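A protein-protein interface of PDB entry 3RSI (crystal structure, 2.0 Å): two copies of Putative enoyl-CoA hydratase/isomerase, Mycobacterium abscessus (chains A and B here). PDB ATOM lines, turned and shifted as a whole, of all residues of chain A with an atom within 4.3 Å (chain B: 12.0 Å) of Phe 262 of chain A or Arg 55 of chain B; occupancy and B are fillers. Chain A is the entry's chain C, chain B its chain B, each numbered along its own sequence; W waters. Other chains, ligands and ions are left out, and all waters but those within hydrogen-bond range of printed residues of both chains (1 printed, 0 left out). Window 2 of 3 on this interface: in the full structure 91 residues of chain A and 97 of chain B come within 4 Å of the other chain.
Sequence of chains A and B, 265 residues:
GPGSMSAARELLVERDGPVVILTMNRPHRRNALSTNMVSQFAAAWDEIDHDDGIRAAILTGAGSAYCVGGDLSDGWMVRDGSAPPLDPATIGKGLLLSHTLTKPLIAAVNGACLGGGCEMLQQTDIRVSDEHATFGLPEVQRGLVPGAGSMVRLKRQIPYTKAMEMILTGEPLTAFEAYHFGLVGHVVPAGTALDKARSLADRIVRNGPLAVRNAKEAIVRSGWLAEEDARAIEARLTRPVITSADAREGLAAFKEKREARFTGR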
ATOM      1  N   PRO A 104      -7.935  -6.813 -19.754  1.00  0.00           N
ATOM      2  CA  PRO A 104      -7.177  -7.616 -20.758  1.00  0.00           C
ATOM      3  C   PRO A 104      -8.100  -8.389 -21.678  1.00  0.00           C
ATOM      4  O   PRO A 104      -9.148  -8.900 -21.220  1.00  0.00           O
ATOM      5  CB  PRO A 104      -6.381  -8.585 -19.895  1.00  0.00           C
ATOM      6  CG  PRO A 104      -6.274  -7.837 -18.547  1.00  0.00           C
ATOM      7  CD  PRO A 104      -7.574  -7.195 -18.378  1.00  0.00           C
ATOM      8  N   ILE A 204      -4.438 -14.271 -15.123  1.00  0.00           N
ATOM      9  CA  ILE A 204      -4.696 -12.839 -15.048  1.00  0.00           C
ATOM     10  C   ILE A 204      -5.725 -12.541 -13.953  1.00  0.00           C
ATOM     11  O   ILE A 204      -5.583 -11.593 -13.204  1.00  0.00           O
ATOM     12  CB  ILE A 204      -5.153 -12.257 -16.418  1.00  0.00           C
ATOM     13  CG1 ILE A 204      -3.990 -12.324 -17.414  1.00  0.00           C
ATOM     14  CG2 ILE A 204      -5.670 -10.808 -16.254  1.00  0.00           C
ATOM     15  CD1 ILE A 204      -4.356 -11.998 -18.839  1.00  0.00           C
ATOM     16  N   VAL A 205      -6.750 -13.383 -13.864  1.00  0.00           N
ATOM     17  CA  VAL A 205      -7.802 -13.249 -12.861  1.00  0.00           C
ATOM     18  C   VAL A 205      -7.272 -13.294 -11.423  1.00  0.00           C
ATOM     19  O   VAL A 205      -7.829 -12.661 -10.532  1.00  0.00           O
ATOM     20  CB  VAL A 205      -8.932 -14.320 -13.140  1.00  0.00           C
ATOM     21  CG1 VAL A 205      -9.554 -14.886 -11.867  1.00  0.00           C
ATOM     22  CG2 VAL A 205      -9.958 -13.705 -14.063  1.00  0.00           C
ATOM     23  N   ARG A 206      -6.181 -14.018 -11.225  1.00  0.00           N
ATOM     24  CA  ARG A 206      -5.553 -14.172  -9.938  1.00  0.00           C
ATOM     25  C   ARG A 206      -4.614 -13.000  -9.625  1.00  0.00           C
ATOM     26  O   ARG A 206      -4.089 -12.903  -8.502  1.00  0.00           O
ATOM     27  CB  ARG A 206      -4.780 -15.499  -9.905  1.00  0.00           C
ATOM     28  CG  ARG A 206      -5.666 -16.761  -9.923  1.00  0.00           C
ATOM     29  CD  ARG A 206      -4.837 -18.007 -10.268  1.00  0.00           C
ATOM     30  NE  ARG A 206      -3.752 -18.194  -9.303  1.00  0.00           N
ATOM     31  CZ  ARG A 206      -2.615 -18.853  -9.525  1.00  0.00           C
ATOM     32  NH1 ARG A 206      -2.361 -19.422 -10.697  1.00  0.00           N
ATOM     33  NH2 ARG A 206      -1.713 -18.940  -8.554  1.00  0.00           N
ATOM     34  N   ASN A 207      -4.410 -12.112 -10.608  1.00  0.00           N
ATOM     35  CA  ASN A 207      -3.541 -10.957 -10.432  1.00  0.00           C
ATOM     36  C   ASN A 207      -4.299  -9.753  -9.912  1.00  0.00           C
ATOM     37  O   ASN A 207      -5.509  -9.699  -9.999  1.00  0.00           O
ATOM     38  CB  ASN A 207      -2.842 -10.612 -11.763  1.00  0.00           C
ATOM     39  CG  ASN A 207      -1.871 -11.681 -12.193  1.00  0.00           C
ATOM     40  OD1 ASN A 207      -1.487 -12.525 -11.392  1.00  0.00           O
ATOM     41  ND2 ASN A 207      -1.455 -11.647 -13.466  1.00  0.00           N
ATOM     42  N   GLY A 208      -3.580  -8.760  -9.408  1.00  0.00           N
ATOM     43  CA  GLY A 208      -4.227  -7.576  -8.826  1.00  0.00           C
ATOM     44  C   GLY A 208      -5.044  -6.798  -9.856  1.00  0.00           C
ATOM     45  O   GLY A 208      -4.493  -6.295 -10.810  1.00  0.00           O
ATOM     46  N   PRO A 209      -6.364  -6.680  -9.662  1.00  0.00           N
ATOM     47  CA  PRO A 209      -7.213  -6.017 -10.682  1.00  0.00           C
ATOM     48  C   PRO A 209      -6.899  -4.546 -10.983  1.00  0.00           C
ATOM     49  O   PRO A 209      -7.018  -4.123 -12.142  1.00  0.00           O
ATOM     50  CB  PRO A 209      -8.612  -6.099 -10.086  1.00  0.00           C
ATOM     51  CG  PRO A 209      -8.552  -7.187  -9.104  1.00  0.00           C
ATOM     52  CD  PRO A 209      -7.168  -7.213  -8.546  1.00  0.00           C
ATOM     53  N   ASP A 246      -4.266  -3.635  -2.240  1.00  0.00           N
ATOM     54  CA  ASP A 246      -3.869  -4.854  -2.971  1.00  0.00           C
ATOM     55  C   ASP A 246      -2.355  -5.041  -3.010  1.00  0.00           C
ATOM     56  O   ASP A 246      -1.877  -6.173  -3.016  1.00  0.00           O
ATOM     57  CB  ASP A 246      -4.396  -4.853  -4.418  1.00  0.00           C
ATOM     58  CG  ASP A 246      -5.842  -5.272  -4.534  1.00  0.00           C
ATOM     59  OD1 ASP A 246      -6.490  -5.625  -3.525  1.00  0.00           O
ATOM     60  OD2 ASP A 246      -6.346  -5.253  -5.678  1.00  0.00           O
ATOM     61  N   GLY A 250      -0.846  -8.367  -1.814  1.00  0.00           N
ATOM     62  CA  GLY A 250      -0.066  -9.105  -2.785  1.00  0.00           C
ATOM     63  C   GLY A 250       1.300  -9.477  -2.256  1.00  0.00           C
ATOM     64  O   GLY A 250       1.719 -10.617  -2.387  1.00  0.00           O
ATOM     65  N   ALA A 260      -3.148 -14.525  -2.919  1.00  0.00           N
ATOM     66  CA  ALA A 260      -3.520 -13.156  -2.635  1.00  0.00           C
ATOM     67  C   ALA A 260      -5.026 -13.044  -2.757  1.00  0.00           C
ATOM     68  O   ALA A 260      -5.620 -13.636  -3.653  1.00  0.00           O
ATOM     69  CB  ALA A 260      -2.851 -12.217  -3.601  1.00  0.00           C
ATOM     70  N   ARG A 261      -5.632 -12.298  -1.837  1.00  0.00           N
ATOM     71  CA  ARG A 261      -7.045 -11.991  -1.886  1.00  0.00           C
ATOM     72  C   ARG A 261      -7.186 -10.516  -2.249  1.00  0.00           C
ATOM     73  O   ARG A 261      -7.186  -9.647  -1.376  1.00  0.00           O
ATOM     74  CB  ARG A 261      -7.688 -12.279  -0.525  1.00  0.00           C
ATOM     75  CG  ARG A 261      -7.645 -13.748  -0.093  1.00  0.00           C
ATOM     76  CD  ARG A 261      -8.829 -14.514  -0.641  1.00  0.00           C
ATOM     77  NE  ARG A 261     -10.076 -14.113   0.019  1.00  0.00           N
ATOM     78  CZ  ARG A 261     -11.249 -14.738  -0.116  1.00  0.00           C
ATOM     79  NH1 ARG A 261     -11.365 -15.813  -0.894  1.00  0.00           N
ATOM     80  NH2 ARG A 261     -12.316 -14.291   0.546  1.00  0.00           N
ATOM     81  N   PHE A 262      -7.306 -10.241  -3.543  1.00  0.00           N
ATOM     82  CA  PHE A 262      -7.321  -8.868  -4.051  1.00  0.00           C
ATOM     83  C   PHE A 262      -8.753  -8.315  -4.116  1.00  0.00           C
ATOM     84  O   PHE A 262      -9.709  -9.073  -4.286  1.00  0.00           O
ATOM     85  CB  PHE A 262      -6.681  -8.798  -5.442  1.00  0.00           C
ATOM     86  CG  PHE A 262      -5.205  -9.129  -5.474  1.00  0.00           C
ATOM     87  CD1 PHE A 262      -4.303  -8.457  -4.662  1.00  0.00           C
ATOM     88  CD2 PHE A 262      -4.710 -10.078  -6.360  1.00  0.00           C
ATOM     89  CE1 PHE A 262      -2.949  -8.737  -4.723  1.00  0.00           C
ATOM     90  CE2 PHE A 262      -3.356 -10.369  -6.407  1.00  0.00           C
ATOM     91  CZ  PHE A 262      -2.479  -9.697  -5.583  1.00  0.00           C
ATOM     92  N   THR A 263      -8.889  -6.999  -3.970  1.00  0.00           N
ATOM     93  CA  THR A 263     -10.182  -6.323  -4.042  1.00  0.00           C
ATOM     94  C   THR A 263     -10.238  -5.201  -5.100  1.00  0.00           C
ATOM     95  O   THR A 263     -11.311  -4.644  -5.357  1.00  0.00           O
ATOM     96  CB  THR A 263     -10.536  -5.685  -2.688  1.00  0.00           C
ATOM     97  OG1 THR A 263      -9.549  -4.698  -2.359  1.00  0.00           O
ATOM     98  CG2 THR A 263     -10.625  -6.755  -1.575  1.00  0.00           C
ATOM     99  N   GLY A 264      -9.104  -4.895  -5.729  1.00  0.00           N
ATOM    100  CA  GLY A 264      -9.012  -3.759  -6.636  1.00  0.00           C
ATOM    101  C   GLY A 264      -8.888  -2.410  -5.937  1.00  0.00           C
ATOM    102  O   GLY A 264      -9.024  -1.372  -6.578  1.00  0.00           O
ATOM    103  N   GLU B  14     -20.713 -15.037 -22.934  1.00  0.00           N
ATOM    104  CA  GLU B  14     -20.787 -16.012 -21.864  1.00  0.00           C
ATOM    105  C   GLU B  14     -19.932 -15.551 -20.677  1.00  0.00           C
ATOM    106  O   GLU B  14     -18.755 -15.220 -20.832  1.00  0.00           O
ATOM    107  CB  GLU B  14     -20.301 -17.371 -22.388  1.00  0.00           C
ATOM    108  CG  GLU B  14     -19.820 -18.359 -21.309  1.00  0.00           C
ATOM    109  CD  GLU B  14     -19.166 -19.611 -21.865  1.00  0.00           C
ATOM    110  OE1 GLU B  14     -19.151 -19.789 -23.108  1.00  0.00           O
ATOM    111  OE2 GLU B  14     -18.670 -20.422 -21.037  1.00  0.00           O
ATOM    112  N   ARG B  15     -20.529 -15.538 -19.488  1.00  0.00           N
ATOM    113  CA  ARG B  15     -19.819 -15.159 -18.255  1.00  0.00           C
ATOM    114  C   ARG B  15     -19.445 -16.419 -17.474  1.00  0.00           C
ATOM    115  O   ARG B  15     -20.324 -17.210 -17.148  1.00  0.00           O
ATOM    116  CB  ARG B  15     -20.725 -14.252 -17.423  1.00  0.00           C
ATOM    117  CG  ARG B  15     -20.137 -13.756 -16.138  1.00  0.00           C
ATOM    118  CD  ARG B  15     -19.162 -12.616 -16.320  1.00  0.00           C
ATOM    119  NE  ARG B  15     -18.783 -12.054 -15.023  1.00  0.00           N
ATOM    120  CZ  ARG B  15     -19.329 -10.980 -14.459  1.00  0.00           C
ATOM    121  NH1 ARG B  15     -20.291 -10.298 -15.060  1.00  0.00           N
ATOM    122  NH2 ARG B  15     -18.896 -10.568 -13.273  1.00  0.00           N
ATOM    123  N   ASP B  16     -18.150 -16.609 -17.205  1.00  0.00           N
ATOM    124  CA  ASP B  16     -17.636 -17.689 -16.347  1.00  0.00           C
ATOM    125  C   ASP B  16     -16.858 -17.072 -15.168  1.00  0.00           C
ATOM    126  O   ASP B  16     -15.631 -16.925 -15.220  1.00  0.00           O
ATOM    127  CB  ASP B  16     -16.712 -18.620 -17.156  1.00  0.00           C
ATOM    128  CG  ASP B  16     -16.146 -19.790 -16.323  1.00  0.00           C
ATOM    129  OD1 ASP B  16     -16.829 -20.244 -15.391  1.00  0.00           O
ATOM    130  OD2 ASP B  16     -15.013 -20.259 -16.608  1.00  0.00           O
ATOM    131  N   GLY B  17     -17.574 -16.699 -14.112  1.00  0.00           N
ATOM    132  CA  GLY B  17     -16.953 -16.014 -12.994  1.00  0.00           C
ATOM    133  C   GLY B  17     -16.354 -14.692 -13.436  1.00  0.00           C
ATOM    134  O   GLY B  17     -17.030 -13.907 -14.085  1.00  0.00           O
ATOM    135  N   PRO B  18     -15.075 -14.438 -13.117  1.00  0.00           N
ATOM    136  CA  PRO B  18     -14.462 -13.167 -13.523  1.00  0.00           C
ATOM    137  C   PRO B  18     -14.067 -13.049 -15.014  1.00  0.00           C
ATOM    138  O   PRO B  18     -13.568 -12.008 -15.425  1.00  0.00           O
ATOM    139  CB  PRO B  18     -13.204 -13.100 -12.655  1.00  0.00           C
ATOM    140  CG  PRO B  18     -12.844 -14.542 -12.432  1.00  0.00           C
ATOM    141  CD  PRO B  18     -14.140 -15.282 -12.354  1.00  0.00           C
ATOM    142  N   VAL B  19     -14.288 -14.100 -15.799  1.00  0.00           N
ATOM    143  CA  VAL B  19     -13.953 -14.119 -17.241  1.00  0.00           C
ATOM    144  C   VAL B  19     -15.227 -14.029 -18.118  1.00  0.00           C
ATOM    145  O   VAL B  19     -16.252 -14.635 -17.808  1.00  0.00           O
ATOM    146  CB  VAL B  19     -13.159 -15.410 -17.578  1.00  0.00           C
ATOM    147  CG1 VAL B  19     -12.709 -15.460 -19.065  1.00  0.00           C
ATOM    148  CG2 VAL B  19     -11.953 -15.545 -16.656  1.00  0.00           C
ATOM    149  N   VAL B  20     -15.167 -13.242 -19.186  1.00  0.00           N
ATOM    150  CA  VAL B  20     -16.219 -13.218 -20.209  1.00  0.00           C
ATOM    151  C   VAL B  20     -15.594 -13.771 -21.477  1.00  0.00           C
ATOM    152  O   VAL B  20     -14.454 -13.421 -21.801  1.00  0.00           O
ATOM    153  CB  VAL B  20     -16.811 -11.782 -20.480  1.00  0.00           C
ATOM    154  CG1 VAL B  20     -15.729 -10.743 -20.520  1.00  0.00           C
ATOM    155  CG2 VAL B  20     -17.583 -11.738 -21.804  1.00  0.00           C
ATOM    156  N   ILE B  21     -16.336 -14.640 -22.166  1.00  0.00           N
ATOM    157  CA  ILE B  21     -15.942 -15.194 -23.444  1.00  0.00           C
ATOM    158  C   ILE B  21     -16.905 -14.692 -24.512  1.00  0.00           C
ATOM    159  O   ILE B  21     -18.127 -14.869 -24.400  1.00  0.00           O
ATOM    160  CB  ILE B  21     -15.979 -16.736 -23.439  1.00  0.00           C
ATOM    161  CG1 ILE B  21     -15.086 -17.288 -22.326  1.00  0.00           C
ATOM    162  CG2 ILE B  21     -15.526 -17.290 -24.802  1.00  0.00           C
ATOM    163  CD1 ILE B  21     -15.471 -18.682 -21.938  1.00  0.00           C
ATOM    164  N   LEU B  22     -16.325 -14.069 -25.533  1.00  0.00           N
ATOM    165  CA  LEU B  22     -17.045 -13.528 -26.660  1.00  0.00           C
ATOM    166  C   LEU B  22     -16.796 -14.442 -27.845  1.00  0.00           C
ATOM    167  O   LEU B  22     -15.640 -14.743 -28.176  1.00  0.00           O
ATOM    168  CB  LEU B  22     -16.524 -12.129 -26.984  1.00  0.00           C
ATOM    169  CG  LEU B  22     -16.630 -11.075 -25.879  1.00  0.00           C
ATOM    170  CD1 LEU B  22     -16.050  -9.755 -26.370  1.00  0.00           C
ATOM    171  CD2 LEU B  22     -18.081 -10.906 -25.477  1.00  0.00           C
ATOM    172  N   ALA B  44     -20.794  -5.060 -25.730  1.00  0.00           N
ATOM    173  CA  ALA B  44     -20.008  -5.981 -24.885  1.00  0.00           C
ATOM    174  C   ALA B  44     -18.800  -5.272 -24.246  1.00  0.00           C
ATOM    175  O   ALA B  44     -18.461  -5.542 -23.101  1.00  0.00           O
ATOM    176  CB  ALA B  44     -19.543  -7.234 -25.697  1.00  0.00           C
ATOM    177  N   TRP B  45     -18.143  -4.387 -24.984  1.00  0.00           N
ATOM    178  CA  TRP B  45     -17.025  -3.627 -24.406  1.00  0.00           C
ATOM    179  C   TRP B  45     -17.521  -2.755 -23.243  1.00  0.00           C
ATOM    180  O   TRP B  45     -16.854  -2.660 -22.215  1.00  0.00           O
ATOM    181  CB  TRP B  45     -16.310  -2.743 -25.435  1.00  0.00           C
ATOM    182  CG  TRP B  45     -15.845  -3.419 -26.699  1.00  0.00           C
ATOM    183  CD1 TRP B  45     -15.952  -2.927 -27.958  1.00  0.00           C
ATOM    184  CD2 TRP B  45     -15.223  -4.706 -26.822  1.00  0.00           C
ATOM    185  NE1 TRP B  45     -15.422  -3.810 -28.862  1.00  0.00           N
ATOM    186  CE2 TRP B  45     -14.963  -4.911 -28.192  1.00  0.00           C
ATOM    187  CE3 TRP B  45     -14.835  -5.692 -25.907  1.00  0.00           C
ATOM    188  CZ2 TRP B  45     -14.357  -6.077 -28.673  1.00  0.00           C
ATOM    189  CZ3 TRP B  45     -14.218  -6.843 -26.384  1.00  0.00           C
ATOM    190  CH2 TRP B  45     -13.976  -7.021 -27.748  1.00  0.00           C
ATOM    191  N   ASP B  46     -18.688  -2.132 -23.407  1.00  0.00           N
ATOM    192  CA  ASP B  46     -19.277  -1.308 -22.346  1.00  0.00           C
ATOM    193  C   ASP B  46     -19.566  -2.128 -21.091  1.00  0.00           C
ATOM    194  O   ASP B  46     -19.248  -1.698 -19.988  1.00  0.00           O
ATOM    195  CB  ASP B  46     -20.545  -0.597 -22.844  1.00  0.00           C
ATOM    196  CG  ASP B  46     -20.230   0.596 -23.732  1.00  0.00           C
ATOM    197  OD1 ASP B  46     -19.065   1.068 -23.755  1.00  0.00           O
ATOM    198  OD2 ASP B  46     -21.144   1.062 -24.420  1.00  0.00           O
ATOM    199  N   GLU B  47     -20.141  -3.316 -21.261  1.00  0.00           N
ATOM    200  CA  GLU B  47     -20.385  -4.242 -20.152  1.00  0.00           C
ATOM    201  C   GLU B  47     -19.093  -4.657 -19.458  1.00  0.00           C
ATOM    202  O   GLU B  47     -19.025  -4.693 -18.234  1.00  0.00           O
ATOM    203  CB  GLU B  47     -21.091  -5.494 -20.666  1.00  0.00           C
ATOM    204  CG  GLU B  47     -21.373  -6.582 -19.618  1.00  0.00           C
ATOM    205  CD  GLU B  47     -22.113  -7.795 -20.224  1.00  0.00           C
ATOM    206  OE1 GLU B  47     -22.975  -7.579 -21.103  1.00  0.00           O
ATOM    207  OE2 GLU B  47     -21.824  -8.963 -19.845  1.00  0.00           O
ATOM    208  N   ILE B  48     -18.075  -4.990 -20.251  1.00  0.00           N
ATOM    209  CA  ILE B  48     -16.785  -5.427 -19.705  1.00  0.00           C
ATOM    210  C   ILE B  48     -16.077  -4.295 -18.952  1.00  0.00           C
ATOM    211  O   ILE B  48     -15.464  -4.522 -17.905  1.00  0.00           O
ATOM    212  CB  ILE B  48     -15.887  -5.976 -20.826  1.00  0.00           C
ATOM    213  CG1 ILE B  48     -16.418  -7.351 -21.285  1.00  0.00           C
ATOM    214  CG2 ILE B  48     -14.428  -6.077 -20.384  1.00  0.00           C
ATOM    215  CD1 ILE B  48     -15.906  -7.748 -22.680  1.00  0.00           C
ATOM    216  N   ASP B  49     -16.169  -3.077 -19.488  1.00  0.00           N
ATOM    217  CA  ASP B  49     -15.531  -1.912 -18.864  1.00  0.00           C
ATOM    218  C   ASP B  49     -16.209  -1.481 -17.560  1.00  0.00           C
ATOM    219  O   ASP B  49     -15.556  -0.991 -16.646  1.00  0.00           O
ATOM    220  CB  ASP B  49     -15.500  -0.726 -19.838  1.00  0.00           C
ATOM    221  CG  ASP B  49     -14.466  -0.893 -20.939  1.00  0.00           C
ATOM    222  OD1 ASP B  49     -13.476  -1.650 -20.753  1.00  0.00           O
ATOM    223  OD2 ASP B  49     -14.644  -0.236 -21.994  1.00  0.00           O
ATOM    224  N   HIS B  50     -17.505  -1.701 -17.460  1.00  0.00           N
ATOM    225  CA  HIS B  50     -18.335  -1.188 -16.359  1.00  0.00           C
ATOM    226  C   HIS B  50     -18.408  -2.141 -15.167  1.00  0.00           C
ATOM    227  O   HIS B  50     -18.592  -1.719 -14.043  1.00  0.00           O
ATOM    228  CB  HIS B  50     -19.757  -0.906 -16.869  1.00  0.00           C
ATOM    229  CG  HIS B  50     -20.703  -0.445 -15.803  1.00  0.00           C
ATOM    230  ND1 HIS B  50     -21.610  -1.288 -15.196  1.00  0.00           N
ATOM    231  CD2 HIS B  50     -20.875   0.768 -15.228  1.00  0.00           C
ATOM    232  CE1 HIS B  50     -22.308  -0.610 -14.303  1.00  0.00           C
ATOM    233  NE2 HIS B  50     -21.878   0.639 -14.300  1.00  0.00           N
ATOM    234  N   ASP B  51     -18.267  -3.436 -15.418  1.00  0.00           N
ATOM    235  CA  ASP B  51     -18.401  -4.418 -14.355  1.00  0.00           C
ATOM    236  C   ASP B  51     -17.035  -4.761 -13.745  1.00  0.00           C
ATOM    237  O   ASP B  51     -16.248  -5.508 -14.333  1.00  0.00           O
ATOM    238  CB  ASP B  51     -19.107  -5.661 -14.888  1.00  0.00           C
ATOM    239  CG  ASP B  51     -19.481  -6.643 -13.795  1.00  0.00           C
ATOM    240  OD1 ASP B  51     -18.940  -6.540 -12.670  1.00  0.00           O
ATOM    241  OD2 ASP B  51     -20.313  -7.533 -14.074  1.00  0.00           O
ATOM    242  N   ASP B  52     -16.771  -4.211 -12.552  1.00  0.00           N
ATOM    243  CA  ASP B  52     -15.516  -4.437 -11.830  1.00  0.00           C
ATOM    244  C   ASP B  52     -15.186  -5.926 -11.606  1.00  0.00           C
ATOM    245  O   ASP B  52     -14.011  -6.288 -11.513  1.00  0.00           O
ATOM    246  CB  ASP B  52     -15.553  -3.729 -10.468  1.00  0.00           C
ATOM    247  CG  ASP B  52     -15.325  -2.226 -10.563  1.00  0.00           C
ATOM    248  OD1 ASP B  52     -14.952  -1.706 -11.640  1.00  0.00           O
ATOM    249  OD2 ASP B  52     -15.503  -1.563  -9.520  1.00  0.00           O
ATOM    250  N   GLY B  53     -16.216  -6.761 -11.499  1.00  0.00           N
ATOM    251  CA  GLY B  53     -16.061  -8.217 -11.347  1.00  0.00           C
ATOM    252  C   GLY B  53     -15.562  -8.944 -12.595  1.00  0.00           C
ATOM    253  O   GLY B  53     -15.141 -10.110 -12.533  1.00  0.00           O
ATOM    254  N   ILE B  54     -15.612  -8.282 -13.743  1.00  0.00           N
ATOM    255  CA  ILE B  54     -15.003  -8.849 -14.946  1.00  0.00           C
ATOM    256  C   ILE B  54     -13.525  -8.469 -14.941  1.00  0.00           C
ATOM    257  O   ILE B  54     -13.193  -7.287 -15.017  1.00  0.00           O
ATOM    258  CB  ILE B  54     -15.685  -8.364 -16.235  1.00  0.00           C
ATOM    259  CG1 ILE B  54     -17.162  -8.770 -16.233  1.00  0.00           C
ATOM    260  CG2 ILE B  54     -14.976  -8.953 -17.454  1.00  0.00           C
ATOM    261  CD1 ILE B  54     -17.915  -8.401 -17.505  1.00  0.00           C
ATOM    262  N   ARG B  55     -12.647  -9.468 -14.842  1.00  0.00           N
ATOM    263  CA  ARG B  55     -11.189  -9.230 -14.798  1.00  0.00           C
ATOM    264  C   ARG B  55     -10.429  -9.552 -16.101  1.00  0.00           C
ATOM    265  O   ARG B  55      -9.277  -9.143 -16.276  1.00  0.00           O
ATOM    266  CB  ARG B  55     -10.583 -10.000 -13.626  1.00  0.00           C
ATOM    267  CG  ARG B  55     -11.030  -9.477 -12.234  1.00  0.00           C
ATOM    268  CD  ARG B  55     -10.238 -10.179 -11.124  1.00  0.00           C
ATOM    269  NE  ARG B  55     -10.699  -9.857  -9.778  1.00  0.00           N
ATOM    270  CZ  ARG B  55     -10.075 -10.215  -8.649  1.00  0.00           C
ATOM    271  NH1 ARG B  55      -8.936 -10.924  -8.677  1.00  0.00           N
ATOM    272  NH2 ARG B  55     -10.583  -9.858  -7.473  1.00  0.00           N
ATOM    273  N   ALA B  56     -11.062 -10.288 -17.009  1.00  0.00           N
ATOM    274  CA  ALA B  56     -10.461 -10.638 -18.285  1.00  0.00           C
ATOM    275  C   ALA B  56     -11.547 -11.034 -19.277  1.00  0.00           C
ATOM    276  O   ALA B  56     -12.600 -11.557 -18.885  1.00  0.00           O
ATOM    277  CB  ALA B  56      -9.459 -11.791 -18.106  1.00  0.00           C
ATOM    278  N   ALA B  57     -11.281 -10.779 -20.555  1.00  0.00           N
ATOM    279  CA  ALA B  57     -12.169 -11.136 -21.646  1.00  0.00           C
ATOM    280  C   ALA B  57     -11.411 -11.956 -22.697  1.00  0.00           C
ATOM    281  O   ALA B  57     -10.230 -11.700 -22.973  1.00  0.00           O
ATOM    282  CB  ALA B  57     -12.726  -9.903 -22.268  1.00  0.00           C
ATOM    283  N   ILE B  58     -12.108 -12.941 -23.265  1.00  0.00           N
ATOM    284  CA  ILE B  58     -11.568 -13.811 -24.298  1.00  0.00           C
ATOM    285  C   ILE B  58     -12.412 -13.653 -25.558  1.00  0.00           C
ATOM    286  O   ILE B  58     -13.650 -13.652 -25.486  1.00  0.00           O
ATOM    287  CB  ILE B  58     -11.572 -15.315 -23.859  1.00  0.00           C
ATOM    288  CG1 ILE B  58     -10.675 -15.521 -22.631  1.00  0.00           C
ATOM    289  CG2 ILE B  58     -11.111 -16.233 -25.030  1.00  0.00           C
ATOM    290  CD1 ILE B  58     -10.776 -16.934 -21.978  1.00  0.00           C
ATOM    291  N   LEU B  59     -11.734 -13.537 -26.697  1.00  0.00           N
ATOM    292  CA  LEU B  59     -12.387 -13.413 -28.000  1.00  0.00           C
ATOM    293  C   LEU B  59     -12.024 -14.586 -28.879  1.00  0.00           C
ATOM    294  O   LEU B  59     -10.836 -14.893 -29.061  1.00  0.00           O
ATOM    295  CB  LEU B  59     -11.961 -12.112 -28.680  1.00  0.00           C
ATOM    296  CG  LEU B  59     -12.615 -11.801 -30.015  1.00  0.00           C
ATOM    297  CD1 LEU B  59     -14.145 -11.828 -29.958  1.00  0.00           C
ATOM    298  CD2 LEU B  59     -12.091 -10.444 -30.485  1.00  0.00           C
HETATM  299  O   HOH W   1      -7.885 -11.946  -5.792  1.00  0.00           O
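No position is printed for both chains.
The backbone NH (N) of Val 20 of chain B is in hydrogen-bond range of the backbone carbonyl oxygen (O) of Ala 56 of chain B (3.1 Å).
The backbone NH (N) of Ala 56 of chain B is in hydrogen-bond range of the backbone carbonyl oxygen (O) of Pro 18 of chain B (3.4 Å).
The backbone NH of Arg 55 of chain B sits at hydrogen-bond distance from the backbone carbonyl oxygen of Pro 18 of chain B, 2.8 Å away.
Of the printed residues of chain A, Arg 55 of chain B touches Pro 104 (3.3 Å), Ile 204 (3.97 Å), Val 205 (2.8 Å), Asn 207 (3.9 Å), Pro 209 (3.4 Å) and Phe 262 (3.4 Å).
Pro 104 of chain A touches just these residues of chain B: Arg 55 (3.3 Å), Ala 56 (3.7 Å) and Ala 57 (2.9 Å).
Asn 207 of chain A touches one residue of chain B.
Of chain B, only Arg 55 (3.4 Å) comes within 4 Å of Pro 209 of chain A.
Ala 260 of chain A touches none of the printed residues of chain B.
No residue of chain B comes within 4 Å of Arg 261 of chain A.
No residue of chain B comes within 4 Å of Thr 263 of chain A.
No residue of chain B comes within 4 Å of Gly 264 of chain A.
Printed residues of chain A within 4 Å of Pro 18 of chain B: Val 205.
Of the printed residues of chain A, Ala 57 of chain B touches Pro 104.
Ile 58 of chain B touches none of the printed residues of chain A.
Water W1 lies within hydrogen-bond range of the backbone NH of Phe 262 of chain A (2.9 Å) and the guanidinium group of Arg 55 of chain B (3.2 Å).
The backbone carbonyl oxygen (O) of Phe 262 of chain A sits at hydrogen-bond distance from the guanidinium group (NH2) of Arg 55 of chain B.
The backbone carbonyl oxygen (O) of Val 205 of chain A lies within hydrogen-bond range of the guanidinium group (NH1) of Arg 55 of chain B, at 2.8 Å.
The backbone NH (N) of Ala 57 of chain B sits at hydrogen-bond distance from the backbone carbonyl oxygen (O) of Pro 104 of chain A (2.9 Å).
CD of Pro 104 of chain A touches O of Arg 55 of chain B, at 3.3 Å.
Ala 56 of chain B touches Pro 104 of chain A (CA to O, 3.7 Å).
Ile 204 of chain A touches Arg 55 of chain B.
Pro 18 of chain B touches Val 205 of chain A (CG to CG1, 3.4 Å).
Val 19 of chain B touches Val 205 of chain A (CG2 to CG2, 3.8 Å).
O of Asn 207 of chain A touches NH1 of Arg 55 of chain B, 3.9 Å away.
CG of Pro 209 of chain A touches CZ of Arg 55 of chain B, 3.4 Å away.
Hydrophobic or aromatic side chains of chain A that line the printed part of chain B: Pro 104, Ile 204, Val 205 and Pro 209.
Of the 25 printed residues of chain B, 5 touch a printed residue of chain A.
Printed residues of chain B that touch a printed residue of chain A: Pro 18, Val 19, Arg 55, Ala 56 and Ala 57.
Among the printed residues, no Asp or Glu carboxylate lies within 4 Å of a Lys or Arg side-chain nitrogen of the other chain.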
